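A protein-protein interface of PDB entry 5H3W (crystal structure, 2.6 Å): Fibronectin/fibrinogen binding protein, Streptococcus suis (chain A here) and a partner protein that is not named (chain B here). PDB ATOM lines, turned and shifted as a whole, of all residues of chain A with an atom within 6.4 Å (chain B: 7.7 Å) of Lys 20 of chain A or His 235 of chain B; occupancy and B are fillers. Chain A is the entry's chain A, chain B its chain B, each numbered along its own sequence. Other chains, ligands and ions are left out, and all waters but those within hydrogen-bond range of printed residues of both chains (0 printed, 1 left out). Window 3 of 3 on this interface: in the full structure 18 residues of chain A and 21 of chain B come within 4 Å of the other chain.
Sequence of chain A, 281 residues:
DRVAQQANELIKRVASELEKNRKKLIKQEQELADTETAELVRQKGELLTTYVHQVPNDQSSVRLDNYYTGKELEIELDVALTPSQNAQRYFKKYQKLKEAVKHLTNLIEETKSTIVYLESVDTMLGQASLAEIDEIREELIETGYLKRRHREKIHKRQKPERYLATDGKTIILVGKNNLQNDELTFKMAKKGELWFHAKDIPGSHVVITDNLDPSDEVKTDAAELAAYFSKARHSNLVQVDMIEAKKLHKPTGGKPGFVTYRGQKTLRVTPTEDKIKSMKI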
ATOM      1  N   ALA A  15      27.231   1.655 -24.368  1.00  0.00           N
ATOM      2  CA  ALA A  15      28.659   1.889 -24.112  1.00  0.00           C
ATOM      3  C   ALA A  15      28.959   3.387 -23.970  1.00  0.00           C
ATOM      4  O   ALA A  15      29.730   3.775 -23.086  1.00  0.00           O
ATOM      5  CB  ALA A  15      29.539   1.250 -25.207  1.00  0.00           C
ATOM      6  N   SER A  16      28.354   4.231 -24.807  1.00  0.00           N
ATOM      7  CA  SER A  16      28.574   5.669 -24.711  1.00  0.00           C
ATOM      8  C   SER A  16      28.053   6.217 -23.400  1.00  0.00           C
ATOM      9  O   SER A  16      28.706   7.030 -22.748  1.00  0.00           O
ATOM     10  CB  SER A  16      27.868   6.405 -25.839  1.00  0.00           C
ATOM     11  OG  SER A  16      28.391   6.019 -27.085  1.00  0.00           O
ATOM     12  N   GLU A  17      26.872   5.767 -23.005  1.00  0.00           N
ATOM     13  CA  GLU A  17      26.314   6.204 -21.739  1.00  0.00           C
ATOM     14  C   GLU A  17      27.220   5.794 -20.560  1.00  0.00           C
ATOM     15  O   GLU A  17      27.470   6.607 -19.658  1.00  0.00           O
ATOM     16  CB  GLU A  17      24.902   5.661 -21.576  1.00  0.00           C
ATOM     17  CG  GLU A  17      23.911   6.340 -22.515  1.00  0.00           C
ATOM     18  CD  GLU A  17      23.839   7.850 -22.322  1.00  0.00           C
ATOM     19  OE1 GLU A  17      23.944   8.308 -21.161  1.00  0.00           O
ATOM     20  OE2 GLU A  17      23.686   8.576 -23.332  1.00  0.00           O
ATOM     21  N   LEU A  18      27.730   4.559 -20.578  1.00  0.00           N
ATOM     22  CA  LEU A  18      28.639   4.107 -19.507  1.00  0.00           C
ATOM     23  C   LEU A  18      29.837   5.033 -19.400  1.00  0.00           C
ATOM     24  O   LEU A  18      30.204   5.486 -18.315  1.00  0.00           O
ATOM     25  CB  LEU A  18      29.118   2.676 -19.746  1.00  0.00           C
ATOM     26  CG  LEU A  18      28.133   1.627 -19.227  1.00  0.00           C
ATOM     27  CD1 LEU A  18      28.524   0.222 -19.669  1.00  0.00           C
ATOM     28  CD2 LEU A  18      28.052   1.719 -17.715  1.00  0.00           C
ATOM     29  N   GLU A  19      30.441   5.306 -20.549  1.00  0.00           N
ATOM     30  CA  GLU A  19      31.599   6.185 -20.610  1.00  0.00           C
ATOM     31  C   GLU A  19      31.235   7.536 -20.057  1.00  0.00           C
ATOM     32  O   GLU A  19      31.988   8.099 -19.279  1.00  0.00           O
ATOM     33  CB  GLU A  19      32.136   6.327 -22.032  1.00  0.00           C
ATOM     34  CG  GLU A  19      33.337   7.219 -22.086  1.00  0.00           C
ATOM     35  CD  GLU A  19      33.821   7.494 -23.492  1.00  0.00           C
ATOM     36  OE1 GLU A  19      32.999   7.432 -24.433  1.00  0.00           O
ATOM     37  OE2 GLU A  19      35.034   7.764 -23.654  1.00  0.00           O
ATOM     38  N   LYS A  20      30.067   8.044 -20.454  1.00  0.00           N
ATOM     39  CA  LYS A  20      29.604   9.365 -20.022  1.00  0.00           C
ATOM     40  C   LYS A  20      29.439   9.399 -18.484  1.00  0.00           C
ATOM     41  O   LYS A  20      29.892  10.341 -17.824  1.00  0.00           O
ATOM     42  CB  LYS A  20      28.306   9.738 -20.757  1.00  0.00           C
ATOM     43  CG  LYS A  20      27.841  11.188 -20.582  1.00  0.00           C
ATOM     44  CD  LYS A  20      26.332  11.366 -20.832  1.00  0.00           C
ATOM     45  CE  LYS A  20      26.041  11.933 -22.238  1.00  0.00           C
ATOM     46  NZ  LYS A  20      24.598  11.853 -22.707  1.00  0.00           N
ATOM     47  N   ASN A  21      28.851   8.360 -17.891  1.00  0.00           N
ATOM     48  CA  ASN A  21      28.658   8.365 -16.436  1.00  0.00           C
ATOM     49  C   ASN A  21      29.909   8.130 -15.591  1.00  0.00           C
ATOM     50  O   ASN A  21      30.001   8.584 -14.429  1.00  0.00           O
ATOM     51  CB  ASN A  21      27.549   7.409 -16.043  1.00  0.00           C
ATOM     52  CG  ASN A  21      26.179   7.950 -16.424  1.00  0.00           C
ATOM     53  OD1 ASN A  21      25.568   8.701 -15.663  1.00  0.00           O
ATOM     54  ND2 ASN A  21      25.704   7.591 -17.613  1.00  0.00           N
ATOM     55  N   ARG A  22      30.877   7.419 -16.157  1.00  0.00           N
ATOM     56  CA  ARG A  22      32.140   7.214 -15.469  1.00  0.00           C
ATOM     57  C   ARG A  22      32.927   8.527 -15.422  1.00  0.00           C
ATOM     58  O   ARG A  22      33.558   8.839 -14.414  1.00  0.00           O
ATOM     59  CB  ARG A  22      32.926   6.109 -16.157  1.00  0.00           C
ATOM     60  CG  ARG A  22      32.349   4.745 -15.860  1.00  0.00           C
ATOM     61  CD  ARG A  22      32.861   3.694 -16.812  1.00  0.00           C
ATOM     62  NE  ARG A  22      32.293   2.398 -16.448  1.00  0.00           N
ATOM     63  CZ  ARG A  22      32.089   1.398 -17.302  1.00  0.00           C
ATOM     64  NH1 ARG A  22      32.412   1.544 -18.591  1.00  0.00           N
ATOM     65  NH2 ARG A  22      31.572   0.252 -16.849  1.00  0.00           N
ATOM     66  N   LYS A  23      32.886   9.299 -16.506  1.00  0.00           N
ATOM     67  CA  LYS A  23      33.503  10.622 -16.523  1.00  0.00           C
ATOM     68  C   LYS A  23      32.804  11.542 -15.510  1.00  0.00           C
ATOM     69  O   LYS A  23      33.425  12.344 -14.799  1.00  0.00           O
ATOM     70  CB  LYS A  23      33.448  11.220 -17.951  1.00  0.00           C
ATOM     71  CG  LYS A  23      34.597  10.715 -18.808  1.00  0.00           C
ATOM     72  CD  LYS A  23      34.548  11.123 -20.260  1.00  0.00           C
ATOM     73  CE  LYS A  23      35.769  10.508 -20.977  1.00  0.00           C
ATOM     74  NZ  LYS A  23      35.766  10.649 -22.456  1.00  0.00           N
ATOM     75  N   LYS A  24      31.496  11.395 -15.437  1.00  0.00           N
ATOM     76  CA  LYS A  24      30.713  12.171 -14.519  1.00  0.00           C
ATOM     77  C   LYS A  24      31.032  11.768 -13.108  1.00  0.00           C
ATOM     78  O   LYS A  24      31.059  12.608 -12.212  1.00  0.00           O
ATOM     79  CB  LYS A  24      29.227  11.962 -14.807  1.00  0.00           C
ATOM     80  CG  LYS A  24      28.312  12.773 -13.937  1.00  0.00           C
ATOM     81  CD  LYS A  24      26.939  12.172 -14.058  1.00  0.00           C
ATOM     82  CE  LYS A  24      25.878  13.050 -13.524  1.00  0.00           C
ATOM     83  NZ  LYS A  24      24.609  12.635 -14.178  1.00  0.00           N
ATOM     84  N   LEU A  25      31.258  10.479 -12.894  1.00  0.00           N
ATOM     85  CA  LEU A  25      31.516  10.003 -11.540  1.00  0.00           C
ATOM     86  C   LEU A  25      32.809  10.550 -10.957  1.00  0.00           C
ATOM     87  O   LEU A  25      32.850  10.983  -9.800  1.00  0.00           O
ATOM     88  CB  LEU A  25      31.537   8.486 -11.486  1.00  0.00           C
ATOM     89  CG  LEU A  25      31.722   8.013 -10.047  1.00  0.00           C
ATOM     90  CD1 LEU A  25      30.556   8.522  -9.182  1.00  0.00           C
ATOM     91  CD2 LEU A  25      31.815   6.515 -10.005  1.00  0.00           C
ATOM     92  N   LYS A  27      34.367  13.228 -11.827  1.00  0.00           N
ATOM     93  CA  LYS A  27      34.225  14.669 -11.673  1.00  0.00           C
ATOM     94  C   LYS A  27      33.518  14.968 -10.354  1.00  0.00           C
ATOM     95  O   LYS A  27      33.947  15.818  -9.577  1.00  0.00           O
ATOM     96  CB  LYS A  27      33.442  15.242 -12.839  1.00  0.00           C
ATOM     97  CG  LYS A  27      34.208  16.227 -13.693  1.00  0.00           C
ATOM     98  CD  LYS A  27      35.482  15.653 -14.253  1.00  0.00           C
ATOM     99  CE  LYS A  27      36.275  16.754 -14.940  1.00  0.00           C
ATOM    100  NZ  LYS A  27      37.613  16.285 -15.363  1.00  0.00           N
ATOM    101  N   GLN A  28      32.459  14.219 -10.081  1.00  0.00           N
ATOM    102  CA  GLN A  28      31.721  14.389  -8.844  1.00  0.00           C
ATOM    103  C   GLN A  28      32.576  14.024  -7.618  1.00  0.00           C
ATOM    104  O   GLN A  28      32.548  14.719  -6.590  1.00  0.00           O
ATOM    105  CB  GLN A  28      30.411  13.593  -8.900  1.00  0.00           C
ATOM    106  CG  GLN A  28      29.447  14.139  -9.948  1.00  0.00           C
ATOM    107  CD  GLN A  28      28.081  13.441  -9.960  1.00  0.00           C
ATOM    108  OE1 GLN A  28      27.981  12.219  -9.800  1.00  0.00           O
ATOM    109  NE2 GLN A  28      27.027  14.223 -10.141  1.00  0.00           N
ATOM    110  N   ILE B 202      18.701  17.857 -27.316  1.00  0.00           N
ATOM    111  CA  ILE B 202      18.755  17.297 -25.955  1.00  0.00           C
ATOM    112  C   ILE B 202      18.473  18.369 -24.896  1.00  0.00           C
ATOM    113  O   ILE B 202      18.655  19.565 -25.151  1.00  0.00           O
ATOM    114  CB  ILE B 202      20.116  16.687 -25.660  1.00  0.00           C
ATOM    115  CG1 ILE B 202      21.151  17.787 -25.669  1.00  0.00           C
ATOM    116  CG2 ILE B 202      20.488  15.622 -26.694  1.00  0.00           C
ATOM    117  CD1 ILE B 202      22.386  17.385 -24.950  1.00  0.00           C
ATOM    118  N   ALA B 228      26.695  23.470 -24.102  1.00  0.00           N
ATOM    119  CA  ALA B 228      26.962  22.033 -24.061  1.00  0.00           C
ATOM    120  C   ALA B 228      27.273  21.589 -22.641  1.00  0.00           C
ATOM    121  O   ALA B 228      26.890  20.490 -22.231  1.00  0.00           O
ATOM    122  CB  ALA B 228      28.084  21.644 -25.005  1.00  0.00           C
ATOM    123  N   TYR B 229      27.977  22.427 -21.883  1.00  0.00           N
ATOM    124  CA  TYR B 229      28.294  22.068 -20.499  1.00  0.00           C
ATOM    125  C   TYR B 229      27.009  21.955 -19.680  1.00  0.00           C
ATOM    126  O   TYR B 229      26.807  20.984 -18.948  1.00  0.00           O
ATOM    127  CB  TYR B 229      29.238  23.086 -19.871  1.00  0.00           C
ATOM    128  CG  TYR B 229      29.729  22.722 -18.481  1.00  0.00           C
ATOM    129  CD1 TYR B 229      30.749  21.785 -18.310  1.00  0.00           C
ATOM    130  CD2 TYR B 229      29.192  23.329 -17.343  1.00  0.00           C
ATOM    131  CE1 TYR B 229      31.216  21.451 -17.053  1.00  0.00           C
ATOM    132  CE2 TYR B 229      29.661  23.010 -16.079  1.00  0.00           C
ATOM    133  CZ  TYR B 229      30.679  22.057 -15.941  1.00  0.00           C
ATOM    134  OH  TYR B 229      31.164  21.714 -14.690  1.00  0.00           O
ATOM    135  N   SER B 231      24.049  20.952 -20.134  1.00  0.00           N
ATOM    136  CA  SER B 231      23.088  20.120 -20.843  1.00  0.00           C
ATOM    137  C   SER B 231      23.259  18.653 -20.463  1.00  0.00           C
ATOM    138  O   SER B 231      24.118  18.302 -19.633  1.00  0.00           O
ATOM    139  CB  SER B 231      23.255  20.291 -22.357  1.00  0.00           C
ATOM    140  OG  SER B 231      24.428  19.647 -22.810  1.00  0.00           O
ATOM    141  N   LYS B 232      22.464  17.793 -21.090  1.00  0.00           N
ATOM    142  CA  LYS B 232      22.528  16.365 -20.814  1.00  0.00           C
ATOM    143  C   LYS B 232      23.788  15.745 -21.444  1.00  0.00           C
ATOM    144  O   LYS B 232      24.117  14.583 -21.172  1.00  0.00           O
ATOM    145  CB  LYS B 232      21.260  15.665 -21.338  1.00  0.00           C
ATOM    146  CG  LYS B 232      20.931  14.332 -20.664  1.00  0.00           C
ATOM    147  CD  LYS B 232      19.794  13.622 -21.360  1.00  0.00           C
ATOM    148  CE  LYS B 232      18.962  12.823 -20.379  1.00  0.00           C
ATOM    149  NZ  LYS B 232      19.841  12.045 -19.469  1.00  0.00           N
ATOM    150  N   ALA B 233      24.501  16.534 -22.257  1.00  0.00           N
ATOM    151  CA  ALA B 233      25.701  16.056 -22.957  1.00  0.00           C
ATOM    152  C   ALA B 233      26.978  16.566 -22.315  1.00  0.00           C
ATOM    153  O   ALA B 233      28.028  16.644 -22.977  1.00  0.00           O
ATOM    154  CB  ALA B 233      25.674  16.458 -24.429  1.00  0.00           C
ATOM    155  N   ARG B 234      26.907  16.897 -21.026  1.00  0.00           N
ATOM    156  CA  ARG B 234      28.042  17.520 -20.346  1.00  0.00           C
ATOM    157  C   ARG B 234      29.363  16.730 -20.455  1.00  0.00           C
ATOM    158  O   ARG B 234      30.403  17.280 -20.857  1.00  0.00           O
ATOM    159  CB  ARG B 234      27.713  17.758 -18.880  1.00  0.00           C
ATOM    160  CG  ARG B 234      28.923  18.086 -18.048  1.00  0.00           C
ATOM    161  CD  ARG B 234      28.521  18.401 -16.633  1.00  0.00           C
ATOM    162  NE  ARG B 234      27.766  19.642 -16.587  1.00  0.00           N
ATOM    163  CZ  ARG B 234      27.506  20.315 -15.474  1.00  0.00           C
ATOM    164  NH1 ARG B 234      27.947  19.858 -14.305  1.00  0.00           N
ATOM    165  NH2 ARG B 234      26.793  21.442 -15.525  1.00  0.00           N
ATOM    166  N   HIS B 235      29.325  15.446 -20.120  1.00  0.00           N
ATOM    167  CA  HIS B 235      30.559  14.659 -20.075  1.00  0.00           C
ATOM    168  C   HIS B 235      30.836  13.805 -21.295  1.00  0.00           C
ATOM    169  O   HIS B 235      31.288  12.687 -21.161  1.00  0.00           O
ATOM    170  CB  HIS B 235      30.568  13.771 -18.840  1.00  0.00           C
ATOM    171  CG  HIS B 235      30.434  14.532 -17.566  1.00  0.00           C
ATOM    172  ND1 HIS B 235      31.478  15.253 -17.019  1.00  0.00           N
ATOM    173  CD2 HIS B 235      29.386  14.684 -16.725  1.00  0.00           C
ATOM    174  CE1 HIS B 235      31.071  15.822 -15.900  1.00  0.00           C
ATOM    175  NE2 HIS B 235      29.806  15.488 -15.695  1.00  0.00           N
ATOM    176  N   SER B 236      30.571  14.323 -22.480  1.00  0.00           N
ATOM    177  CA  SER B 236      30.783  13.566 -23.698  1.00  0.00           C
ATOM    178  C   SER B 236      31.591  14.447 -24.644  1.00  0.00           C
ATOM    179  O   SER B 236      31.677  15.654 -24.424  1.00  0.00           O
ATOM    180  CB  SER B 236      29.424  13.169 -24.312  1.00  0.00           C
ATOM    181  OG  SER B 236      28.739  14.276 -24.893  1.00  0.00           O
ATOM    182  N   ASN B 237      32.212  13.873 -25.673  1.00  0.00           N
ATOM    183  CA  ASN B 237      32.975  14.705 -26.608  1.00  0.00           C
ATOM    184  C   ASN B 237      32.132  15.184 -27.792  1.00  0.00           C
ATOM    185  O   ASN B 237      31.035  14.671 -28.034  1.00  0.00           O
ATOM    186  CB  ASN B 237      34.224  13.983 -27.104  1.00  0.00           C
ATOM    187  CG  ASN B 237      35.150  13.593 -25.977  1.00  0.00           C
ATOM    188  OD1 ASN B 237      36.077  14.332 -25.639  1.00  0.00           O
ATOM    189  ND2 ASN B 237      34.921  12.415 -25.400  1.00  0.00           N
ATOM    190  N   VAL B 239      29.994  17.835 -28.783  1.00  0.00           N
ATOM    191  CA  VAL B 239      28.575  18.105 -28.640  1.00  0.00           C
ATOM    192  C   VAL B 239      28.128  19.109 -29.689  1.00  0.00           C
ATOM    193  O   VAL B 239      28.789  20.121 -29.895  1.00  0.00           O
ATOM    194  CB  VAL B 239      28.286  18.698 -27.261  1.00  0.00           C
ATOM    195  CG1 VAL B 239      26.792  18.818 -27.036  1.00  0.00           C
ATOM    196  CG2 VAL B 239      28.933  17.841 -26.169  1.00  0.00           C
ATOM    197  N   THR B 271      33.672  20.858 -27.189  1.00  0.00           N
ATOM    198  CA  THR B 271      33.878  19.924 -26.083  1.00  0.00           C
ATOM    199  C   THR B 271      34.051  20.732 -24.806  1.00  0.00           C
ATOM    200  O   THR B 271      35.081  21.361 -24.593  1.00  0.00           O
ATOM    201  CB  THR B 271      35.099  19.022 -26.307  1.00  0.00           C
ATOM    202  OG1 THR B 271      35.023  18.432 -27.612  1.00  0.00           O
ATOM    203  CG2 THR B 271      35.155  17.939 -25.254  1.00  0.00           C
ATOM    204  N   PRO B 272      33.027  20.742 -23.959  1.00  0.00           N
ATOM    205  CA  PRO B 272      33.109  21.558 -22.748  1.00  0.00           C
ATOM    206  C   PRO B 272      34.190  21.023 -21.804  1.00  0.00           C
ATOM    207  O   PRO B 272      34.442  19.822 -21.744  1.00  0.00           O
ATOM    208  CB  PRO B 272      31.730  21.379 -22.109  1.00  0.00           C
ATOM    209  CG  PRO B 272      30.873  20.786 -23.177  1.00  0.00           C
ATOM    210  CD  PRO B 272      31.780  19.971 -24.024  1.00  0.00           C
ATOM    211  N   GLU B 274      35.414  21.542 -17.707  1.00  0.00           N
ATOM    212  CA  GLU B 274      35.203  22.095 -16.367  1.00  0.00           C
ATOM    213  C   GLU B 274      36.141  23.248 -16.033  1.00  0.00           C
ATOM    214  O   GLU B 274      35.750  24.190 -15.364  1.00  0.00           O
ATOM    215  CB  GLU B 274      35.346  21.012 -15.298  1.00  0.00           C
ATOM    216  CG  GLU B 274      34.929  21.469 -13.912  1.00  0.00           C
ATOM    217  CD  GLU B 274      34.881  20.334 -12.912  1.00  0.00           C
ATOM    218  OE1 GLU B 274      35.679  19.380 -13.051  1.00  0.00           O
ATOM    219  OE2 GLU B 274      34.046  20.392 -11.985  1.00  0.00           O
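His 235 of chain B touches Lys 20 of chain A (CB to O, 3.6 Å). His 235 of chain B touches Lys 23 of chain A (O to CD, 3.7 Å). Asn 237 of chain B touches Lys 23 of chain A (ND2 to NZ, 3.5 Å). His 235 of chain B touches Lys 24 of chain A (CD2 to CB, 3.3 Å). Lys 27 of chain A touches His 235 of chain B (CG to CE1, 3.9 Å). OE1 of Glu 274 of chain B touches CE of Lys 27 of chain A, 3.3 Å away.
Of chain B, only Lys 232 and His 235 come within 4 Å of Lys 20 of chain A. Of the printed residues of chain A, Lys 232 of chain B touches Lys 20 (3.2 Å). Ser 236 of chain B touches none of the printed residues of chain A. Printed residues of chain A within 4 Å of Asn 237 of chain B: Lys 23 (3.5 Å). The nearest residue of chain B that does not touch Lys 20 of chain A is Ser 236 of chain B (4.2 Å). The nearest printed residue of chain B that does not touch Lys 24 of chain A is Arg 234 of chain B (6.2 Å).
Printed residues of chain A that touch a printed residue of chain B: Lys 20, Lys 23, Lys 24 and Lys 27. Along chain A the printed residues that touch a printed residue of chain B span positions 20 to 27. Of the 14 printed residues of chain B, 4 touch a printed residue of chain A. Among the printed residues, 7 pairs touch across the chains.
The side-chain carboxylate (OE2) of Glu 17 of chain A lies within salt-bridge range of the side-chain amino group (NZ) of Lys 20 of chain A (3.5 Å). The side-chain carboxylate of Glu 19 of chain A is in salt-bridge range of the side-chain amino group of Lys 23 of chain A, 3.2 Å away.
NZ of Lys 20 of chain A is in hydrogen-bond range of O of Lys 232 of chain B (3.2 Å).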
